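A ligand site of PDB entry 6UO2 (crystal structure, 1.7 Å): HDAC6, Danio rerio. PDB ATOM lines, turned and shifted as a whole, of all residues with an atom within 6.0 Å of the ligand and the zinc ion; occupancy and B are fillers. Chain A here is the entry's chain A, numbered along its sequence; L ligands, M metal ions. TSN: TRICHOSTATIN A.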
ATOM      1  N   TRP A  25     -17.108 -13.385 -13.811  1.00  0.00           N
ATOM      2  CA  TRP A  25     -18.013 -13.716 -12.730  1.00  0.00           C
ATOM      3  C   TRP A  25     -17.339 -13.695 -11.365  1.00  0.00           C
ATOM      4  O   TRP A  25     -17.976 -14.062 -10.366  1.00  0.00           O
ATOM      5  CB  TRP A  25     -18.675 -15.078 -12.969  1.00  0.00           C
ATOM      6  CG  TRP A  25     -17.764 -16.146 -13.537  1.00  0.00           C
ATOM      7  CD1 TRP A  25     -17.579 -16.457 -14.854  1.00  0.00           C
ATOM      8  CD2 TRP A  25     -16.955 -17.066 -12.792  1.00  0.00           C
ATOM      9  NE1 TRP A  25     -16.701 -17.504 -14.978  1.00  0.00           N
ATOM     10  CE2 TRP A  25     -16.293 -17.892 -13.722  1.00  0.00           C
ATOM     11  CE3 TRP A  25     -16.717 -17.266 -11.423  1.00  0.00           C
ATOM     12  CZ2 TRP A  25     -15.410 -18.906 -13.340  1.00  0.00           C
ATOM     13  CZ3 TRP A  25     -15.837 -18.276 -11.050  1.00  0.00           C
ATOM     14  CH2 TRP A  25     -15.196 -19.077 -11.998  1.00  0.00           C
ATOM     15  N   ASP A  26     -16.088 -13.238 -11.278  1.00  0.00           N
ATOM     16  CA  ASP A  26     -15.385 -13.160  -9.997  1.00  0.00           C
ATOM     17  C   ASP A  26     -14.307 -12.079 -10.123  1.00  0.00           C
ATOM     18  O   ASP A  26     -13.258 -12.316 -10.720  1.00  0.00           O
ATOM     19  CB  ASP A  26     -14.781 -14.499  -9.613  1.00  0.00           C
ATOM     20  CG  ASP A  26     -14.047 -14.460  -8.278  1.00  0.00           C
ATOM     21  OD1 ASP A  26     -13.993 -13.387  -7.633  1.00  0.00           O
ATOM     22  OD2 ASP A  26     -13.505 -15.518  -7.859  1.00  0.00           O
ATOM     23  N   HIS A  29     -10.799 -13.103  -8.737  1.00  0.00           N
ATOM     24  CA  HIS A  29     -10.172 -14.336  -9.197  1.00  0.00           C
ATOM     25  C   HIS A  29      -8.655 -14.224  -9.076  1.00  0.00           C
ATOM     26  O   HIS A  29      -8.093 -13.146  -9.348  1.00  0.00           O
ATOM     27  CB  HIS A  29     -10.571 -14.625 -10.656  1.00  0.00           C
ATOM     28  CG  HIS A  29     -10.329 -16.031 -11.073  1.00  0.00           C
ATOM     29  ND1 HIS A  29      -9.070 -16.508 -11.384  1.00  0.00           N
ATOM     30  CD2 HIS A  29     -11.169 -17.082 -11.226  1.00  0.00           C
ATOM     31  CE1 HIS A  29      -9.158 -17.788 -11.714  1.00  0.00           C
ATOM     32  NE2 HIS A  29     -10.419 -18.158 -11.624  1.00  0.00           N
ATOM     33  N   PRO A  30      -7.961 -15.284  -8.663  1.00  0.00           N
ATOM     34  CA  PRO A  30      -6.506 -15.169  -8.471  1.00  0.00           C
ATOM     35  C   PRO A  30      -5.735 -14.974  -9.755  1.00  0.00           C
ATOM     36  O   PRO A  30      -4.658 -14.368  -9.721  1.00  0.00           O
ATOM     37  CB  PRO A  30      -6.144 -16.498  -7.790  1.00  0.00           C
ATOM     38  CG  PRO A  30      -7.200 -17.452  -8.225  1.00  0.00           C
ATOM     39  CD  PRO A  30      -8.469 -16.656  -8.406  1.00  0.00           C
ATOM     40  N   ASP A  96     -11.642 -28.337 -16.155  1.00  0.00           N
ATOM     41  CA  ASP A  96     -11.221 -28.270 -14.764  1.00  0.00           C
ATOM     42  C   ASP A  96     -10.518 -26.941 -14.504  1.00  0.00           C
ATOM     43  O   ASP A  96      -9.448 -26.672 -15.079  1.00  0.00           O
ATOM     44  CB  ASP A  96     -10.292 -29.443 -14.431  1.00  0.00           C
ATOM     45  CG  ASP A  96      -9.805 -29.404 -12.990  1.00  0.00           C
ATOM     46  OD1 ASP A  96     -10.298 -28.568 -12.209  1.00  0.00           O
ATOM     47  OD2 ASP A  96      -8.916 -30.218 -12.655  1.00  0.00           O
ATOM     48  N   SER A  97     -11.117 -26.106 -13.653  1.00  0.00           N
ATOM     49  CA  SER A  97     -10.509 -24.886 -13.114  1.00  0.00           C
ATOM     50  C   SER A  97     -10.061 -23.929 -14.216  1.00  0.00           C
ATOM     51  O   SER A  97      -8.884 -23.602 -14.356  1.00  0.00           O
ATOM     52  CB  SER A  97      -9.330 -25.235 -12.192  1.00  0.00           C
ATOM     53  OG  SER A  97      -9.738 -26.056 -11.115  1.00  0.00           O
ATOM     54  N   VAL A  98     -11.030 -23.429 -14.980  1.00  0.00           N
ATOM     55  CA  VAL A  98     -10.788 -22.365 -15.946  1.00  0.00           C
ATOM     56  C   VAL A  98     -11.937 -21.374 -15.918  1.00  0.00           C
ATOM     57  O   VAL A  98     -13.042 -21.678 -15.447  1.00  0.00           O
ATOM     58  CB  VAL A  98     -10.587 -22.877 -17.398  1.00  0.00           C
ATOM     59  CG1 VAL A  98      -9.521 -23.958 -17.461  1.00  0.00           C
ATOM     60  CG2 VAL A  98     -11.887 -23.369 -17.960  1.00  0.00           C
ATOM     61  N   HIS A 139       1.095 -24.414 -18.882  1.00  0.00           N
ATOM     62  CA  HIS A 139       1.636 -25.763 -18.727  1.00  0.00           C
ATOM     63  C   HIS A 139       0.592 -26.829 -18.428  1.00  0.00           C
ATOM     64  O   HIS A 139       0.934 -28.013 -18.435  1.00  0.00           O
ATOM     65  CB  HIS A 139       2.770 -25.809 -17.679  1.00  0.00           C
ATOM     66  CG  HIS A 139       2.369 -25.485 -16.269  1.00  0.00           C
ATOM     67  ND1 HIS A 139       3.074 -25.961 -15.188  1.00  0.00           N
ATOM     68  CD2 HIS A 139       1.414 -24.663 -15.751  1.00  0.00           C
ATOM     69  CE1 HIS A 139       2.564 -25.504 -14.063  1.00  0.00           C
ATOM     70  NE2 HIS A 139       1.558 -24.693 -14.381  1.00  0.00           N
ATOM     71  N   HIS A 140      -0.677 -26.452 -18.185  1.00  0.00           N
ATOM     72  CA  HIS A 140      -1.749 -27.432 -18.033  1.00  0.00           C
ATOM     73  C   HIS A 140      -2.565 -27.647 -19.303  1.00  0.00           C
ATOM     74  O   HIS A 140      -3.293 -28.642 -19.375  1.00  0.00           O
ATOM     75  CB  HIS A 140      -2.727 -27.024 -16.918  1.00  0.00           C
ATOM     76  CG  HIS A 140      -2.062 -26.761 -15.613  1.00  0.00           C
ATOM     77  ND1 HIS A 140      -1.323 -27.709 -14.950  1.00  0.00           N
ATOM     78  CD2 HIS A 140      -2.008 -25.643 -14.852  1.00  0.00           C
ATOM     79  CE1 HIS A 140      -0.851 -27.197 -13.831  1.00  0.00           C
ATOM     80  NE2 HIS A 140      -1.266 -25.942 -13.746  1.00  0.00           N
ATOM     81  N   GLY A 148      -6.803 -25.675 -15.918  1.00  0.00           N
ATOM     82  CA  GLY A 148      -6.055 -24.965 -14.893  1.00  0.00           C
ATOM     83  C   GLY A 148      -5.602 -23.583 -15.309  1.00  0.00           C
ATOM     84  O   GLY A 148      -4.423 -23.248 -15.204  1.00  0.00           O
ATOM     85  N   PHE A 149      -6.534 -22.782 -15.814  1.00  0.00           N
ATOM     86  CA  PHE A 149      -6.314 -21.392 -16.212  1.00  0.00           C
ATOM     87  C   PHE A 149      -5.567 -21.264 -17.538  1.00  0.00           C
ATOM     88  O   PHE A 149      -5.212 -20.137 -17.937  1.00  0.00           O
ATOM     89  CB  PHE A 149      -5.532 -20.593 -15.162  1.00  0.00           C
ATOM     90  CG  PHE A 149      -6.085 -20.704 -13.768  1.00  0.00           C
ATOM     91  CD1 PHE A 149      -7.428 -20.914 -13.542  1.00  0.00           C
ATOM     92  CD2 PHE A 149      -5.237 -20.588 -12.664  1.00  0.00           C
ATOM     93  CE1 PHE A 149      -7.929 -21.015 -12.256  1.00  0.00           C
ATOM     94  CE2 PHE A 149      -5.725 -20.683 -11.379  1.00  0.00           C
ATOM     95  CZ  PHE A 149      -7.089 -20.901 -11.173  1.00  0.00           C
ATOM     96  N   ASP A 177       7.092 -24.225 -11.272  1.00  0.00           N
ATOM     97  CA  ASP A 177       5.782 -23.886 -10.714  1.00  0.00           C
ATOM     98  C   ASP A 177       5.389 -24.926  -9.668  1.00  0.00           C
ATOM     99  O   ASP A 177       5.759 -26.095  -9.764  1.00  0.00           O
ATOM    100  CB  ASP A 177       4.764 -23.832 -11.876  1.00  0.00           C
ATOM    101  CG  ASP A 177       3.410 -23.315 -11.460  1.00  0.00           C
ATOM    102  OD1 ASP A 177       2.691 -24.073 -10.808  1.00  0.00           O
ATOM    103  OD2 ASP A 177       3.057 -22.165 -11.793  1.00  0.00           O
ATOM    104  N   VAL A 178       4.639 -24.491  -8.645  1.00  0.00           N
ATOM    105  CA  VAL A 178       4.305 -25.428  -7.575  1.00  0.00           C
ATOM    106  C   VAL A 178       3.327 -26.506  -8.032  1.00  0.00           C
ATOM    107  O   VAL A 178       3.157 -27.524  -7.331  1.00  0.00           O
ATOM    108  CB  VAL A 178       3.732 -24.681  -6.367  1.00  0.00           C
ATOM    109  CG1 VAL A 178       2.243 -24.391  -6.575  1.00  0.00           C
ATOM    110  CG2 VAL A 178       3.975 -25.476  -5.093  1.00  0.00           C
ATOM    111  N   HIS A 179       2.664 -26.319  -9.167  1.00  0.00           N
ATOM    112  CA  HIS A 179       1.748 -27.325  -9.691  1.00  0.00           C
ATOM    113  C   HIS A 179       2.421 -28.158 -10.768  1.00  0.00           C
ATOM    114  O   HIS A 179       3.306 -27.686 -11.495  1.00  0.00           O
ATOM    115  CB  HIS A 179       0.490 -26.689 -10.264  1.00  0.00           C
ATOM    116  CG  HIS A 179      -0.243 -25.841  -9.275  1.00  0.00           C
ATOM    117  ND1 HIS A 179      -0.068 -24.466  -9.206  1.00  0.00           N
ATOM    118  CD2 HIS A 179      -1.146 -26.159  -8.322  1.00  0.00           C
ATOM    119  CE1 HIS A 179      -0.828 -23.989  -8.240  1.00  0.00           C
ATOM    120  NE2 HIS A 179      -1.500 -24.991  -7.692  1.00  0.00           N
ATOM    121  N   TRP A 208      -4.096 -30.223  -6.051  1.00  0.00           N
ATOM    122  CA  TRP A 208      -4.469 -30.120  -7.444  1.00  0.00           C
ATOM    123  C   TRP A 208      -3.208 -30.211  -8.302  1.00  0.00           C
ATOM    124  O   TRP A 208      -2.187 -29.618  -7.951  1.00  0.00           O
ATOM    125  CB  TRP A 208      -5.207 -28.796  -7.669  1.00  0.00           C
ATOM    126  CG  TRP A 208      -5.805 -28.699  -9.009  1.00  0.00           C
ATOM    127  CD1 TRP A 208      -7.062 -29.065  -9.368  1.00  0.00           C
ATOM    128  CD2 TRP A 208      -5.157 -28.236 -10.205  1.00  0.00           C
ATOM    129  NE1 TRP A 208      -7.247 -28.859 -10.716  1.00  0.00           N
ATOM    130  CE2 TRP A 208      -6.091 -28.349 -11.243  1.00  0.00           C
ATOM    131  CE3 TRP A 208      -3.880 -27.733 -10.480  1.00  0.00           C
ATOM    132  CZ2 TRP A 208      -5.790 -27.998 -12.548  1.00  0.00           C
ATOM    133  CZ3 TRP A 208      -3.591 -27.372 -11.767  1.00  0.00           C
ATOM    134  CH2 TRP A 208      -4.528 -27.509 -12.792  1.00  0.00           C
ATOM    135  N   GLY A 268       6.709 -20.545 -12.958  1.00  0.00           N
ATOM    136  CA  GLY A 268       5.701 -20.098 -12.018  1.00  0.00           C
ATOM    137  C   GLY A 268       6.347 -19.746 -10.686  1.00  0.00           C
ATOM    138  O   GLY A 268       7.460 -20.176 -10.371  1.00  0.00           O
ATOM    139  N   ASP A 270       4.406 -19.672  -7.609  1.00  0.00           N
ATOM    140  CA  ASP A 270       3.511 -20.004  -6.498  1.00  0.00           C
ATOM    141  C   ASP A 270       4.147 -20.926  -5.469  1.00  0.00           C
ATOM    142  O   ASP A 270       3.458 -21.355  -4.535  1.00  0.00           O
ATOM    143  CB  ASP A 270       2.180 -20.572  -7.025  1.00  0.00           C
ATOM    144  CG  ASP A 270       2.339 -21.446  -8.275  1.00  0.00           C
ATOM    145  OD1 ASP A 270       3.462 -21.890  -8.594  1.00  0.00           O
ATOM    146  OD2 ASP A 270       1.309 -21.656  -8.951  1.00  0.00           O
ATOM    147  N   LYS A 277      -1.816 -19.974  -1.881  1.00  0.00           N
ATOM    148  CA  LYS A 277      -2.275 -21.350  -2.033  1.00  0.00           C
ATOM    149  C   LYS A 277      -1.171 -22.367  -2.257  1.00  0.00           C
ATOM    150  O   LYS A 277      -1.422 -23.565  -2.065  1.00  0.00           O
ATOM    151  CB  LYS A 277      -3.274 -21.457  -3.195  1.00  0.00           C
ATOM    152  N   GLU A 307       4.278 -18.831 -15.596  1.00  0.00           N
ATOM    153  CA  GLU A 307       3.132 -19.708 -15.397  1.00  0.00           C
ATOM    154  C   GLU A 307       2.307 -19.174 -14.229  1.00  0.00           C
ATOM    155  O   GLU A 307       1.744 -18.084 -14.334  1.00  0.00           O
ATOM    156  CB  GLU A 307       3.592 -21.157 -15.171  1.00  0.00           C
ATOM    157  CG  GLU A 307       4.415 -21.748 -16.328  1.00  0.00           C
ATOM    158  CD  GLU A 307       3.568 -22.158 -17.532  1.00  0.00           C
ATOM    159  OE1 GLU A 307       4.121 -22.595 -18.551  1.00  0.00           O
ATOM    160  OE2 GLU A 307       2.325 -22.039 -17.470  1.00  0.00           O
ATOM    161  N   GLY A 308       2.240 -19.894 -13.111  1.00  0.00           N
ATOM    162  CA  GLY A 308       1.452 -19.466 -11.971  1.00  0.00           C
ATOM    163  C   GLY A 308       2.209 -18.538 -11.031  1.00  0.00           C
ATOM    164  O   GLY A 308       3.276 -18.000 -11.338  1.00  0.00           O
ATOM    165  N   GLY A 309       1.625 -18.334  -9.850  1.00  0.00           N
ATOM    166  CA  GLY A 309       2.156 -17.408  -8.865  1.00  0.00           C
ATOM    167  C   GLY A 309       1.145 -16.307  -8.633  1.00  0.00           C
ATOM    168  O   GLY A 309       0.853 -15.529  -9.540  1.00  0.00           O
ATOM    169  N   TYR A 310       0.568 -16.254  -7.435  1.00  0.00           N
ATOM    170  CA  TYR A 310      -0.638 -15.459  -7.226  1.00  0.00           C
ATOM    171  C   TYR A 310      -0.533 -14.416  -6.111  1.00  0.00           C
ATOM    172  O   TYR A 310      -1.463 -13.623  -5.961  1.00  0.00           O
ATOM    173  CB  TYR A 310      -1.828 -16.400  -6.974  1.00  0.00           C
ATOM    174  CG  TYR A 310      -1.980 -17.341  -8.148  1.00  0.00           C
ATOM    175  CD1 TYR A 310      -2.621 -16.935  -9.305  1.00  0.00           C
ATOM    176  CD2 TYR A 310      -1.387 -18.606  -8.128  1.00  0.00           C
ATOM    177  CE1 TYR A 310      -2.726 -17.773 -10.398  1.00  0.00           C
ATOM    178  CE2 TYR A 310      -1.484 -19.460  -9.218  1.00  0.00           C
ATOM    179  CZ  TYR A 310      -2.165 -19.035 -10.346  1.00  0.00           C
ATOM    180  OH  TYR A 310      -2.277 -19.858 -11.442  1.00  0.00           O
HETATM  181  O1  TSN L   1       0.374 -23.438 -12.092  1.00  0.00           O
HETATM  182  O2  TSN L   1      -1.184 -22.113 -10.561  1.00  0.00           O
HETATM  183  O3  TSN L   1      -7.465 -22.277  -6.941  1.00  0.00           O
HETATM  184  N1  TSN L   1      -0.936 -23.696 -12.134  1.00  0.00           N
HETATM  185  N2  TSN L   1     -13.255 -21.829  -9.683  1.00  0.00           N
HETATM  186  C1  TSN L   1      -9.361 -22.539  -8.331  1.00  0.00           C
HETATM  187  C2  TSN L   1     -10.037 -23.468  -9.105  1.00  0.00           C
HETATM  188  C3  TSN L   1     -11.319 -23.235  -9.550  1.00  0.00           C
HETATM  189  C4  TSN L   1     -11.960 -22.038  -9.221  1.00  0.00           C
HETATM  190  C5  TSN L   1     -11.288 -21.068  -8.430  1.00  0.00           C
HETATM  191  C6  TSN L   1      -9.996 -21.337  -7.990  1.00  0.00           C
HETATM  192  C7  TSN L   1      -7.981 -22.854  -7.886  1.00  0.00           C
HETATM  193  C8  TSN L   1      -7.206 -23.956  -8.619  1.00  0.00           C
HETATM  194  C9  TSN L   1      -5.777 -23.574  -8.867  1.00  0.00           C
HETATM  195  C10 TSN L   1      -5.167 -23.707 -10.061  1.00  0.00           C
HETATM  196  C11 TSN L   1      -3.768 -23.330 -10.172  1.00  0.00           C
HETATM  197  C12 TSN L   1      -3.118 -23.301 -11.325  1.00  0.00           C
HETATM  198  C13 TSN L   1      -1.705 -22.950 -11.284  1.00  0.00           C
HETATM  199  C14 TSN L   1      -7.223 -25.229  -7.811  1.00  0.00           C
HETATM  200  C15 TSN L   1      -5.820 -24.236 -11.304  1.00  0.00           C
HETATM  201  C17 TSN L   1     -13.604 -22.207 -11.056  1.00  0.00           C
HETATM  202  C16 TSN L   1     -14.309 -21.273  -8.834  1.00  0.00           C
HETATM  203 ZN    ZN M   1       0.958 -23.123 -10.385  1.00  0.00          ZN
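Residues that only touch the ligand: Ser 97 (3.3 Å), Phe 149 (3.3 Å), Trp 25 (3.6 Å), Gly 148 (3.7 Å), Trp 208 (3.8 Å) and Gly 308 (3.99 Å).
12 residues have an atom within 4 Å of the ligand: Trp 25, Ser 97, His 139, His 140, Gly 148, Phe 149, Asp 177, His 179, Trp 208, Asp 270, Gly 308 and Tyr 310.
An oxygen (O2) of the ligand sits close to the side-chain hydroxyl (OH) of Tyr 310 (2.7 Å).
A ring nitrogen (NE2) of His 140 is in hydrogen-bond range of a nitrogen (N1) of the ligand.
NE2 of His 139 lies close to O1 of the ligand (2.9 Å).
Of the 22 residues printed, 3 come within 4 Å of the zinc ion.
The backbone NH of Gly 308 sits at hydrogen-bond distance from the side-chain carboxylate of Asp 177, at 2.7 Å.
OD1 of Asp 270 is in hydrogen-bond range of N of Val 178.
OD2 of Asp 270 lies close to N of Gly 309, at 3.5 Å.
NE2 of His 140 lies within hydrogen-bond range of NE2 of His 139 (3.2 Å).
N of His 139 lies within hydrogen-bond range of OE2 of Glu 307, 3.0 Å away.
The backbone carbonyl oxygen of Ser 97 sits close to the backbone NH of Gly 148, 3.3 Å away.
O of Asp 96 lies within hydrogen-bond range of N of Gly 148.
The side-chain carboxylate (OD2) of Asp 96 lies within hydrogen-bond range of the indole nitrogen (NE1) of Trp 208 (2.9 Å).
The zinc ion is bound by an oxygen (O1) of the ligand, at 1.8 Å.
The zinc ion is bound by OD1 of Asp 177.
The zinc ion is bound by ND1 of His 179, 2.1 Å away.
The zinc ion is bound by OD2 of Asp 270 (2.1 Å).
The zinc ion is bound by O2 of the ligand (2.4 Å).
The zinc ion has five donor atoms within binding distance.
Slightly farther from the zinc ion lies OD2 of Asp 177 (2.7 Å).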
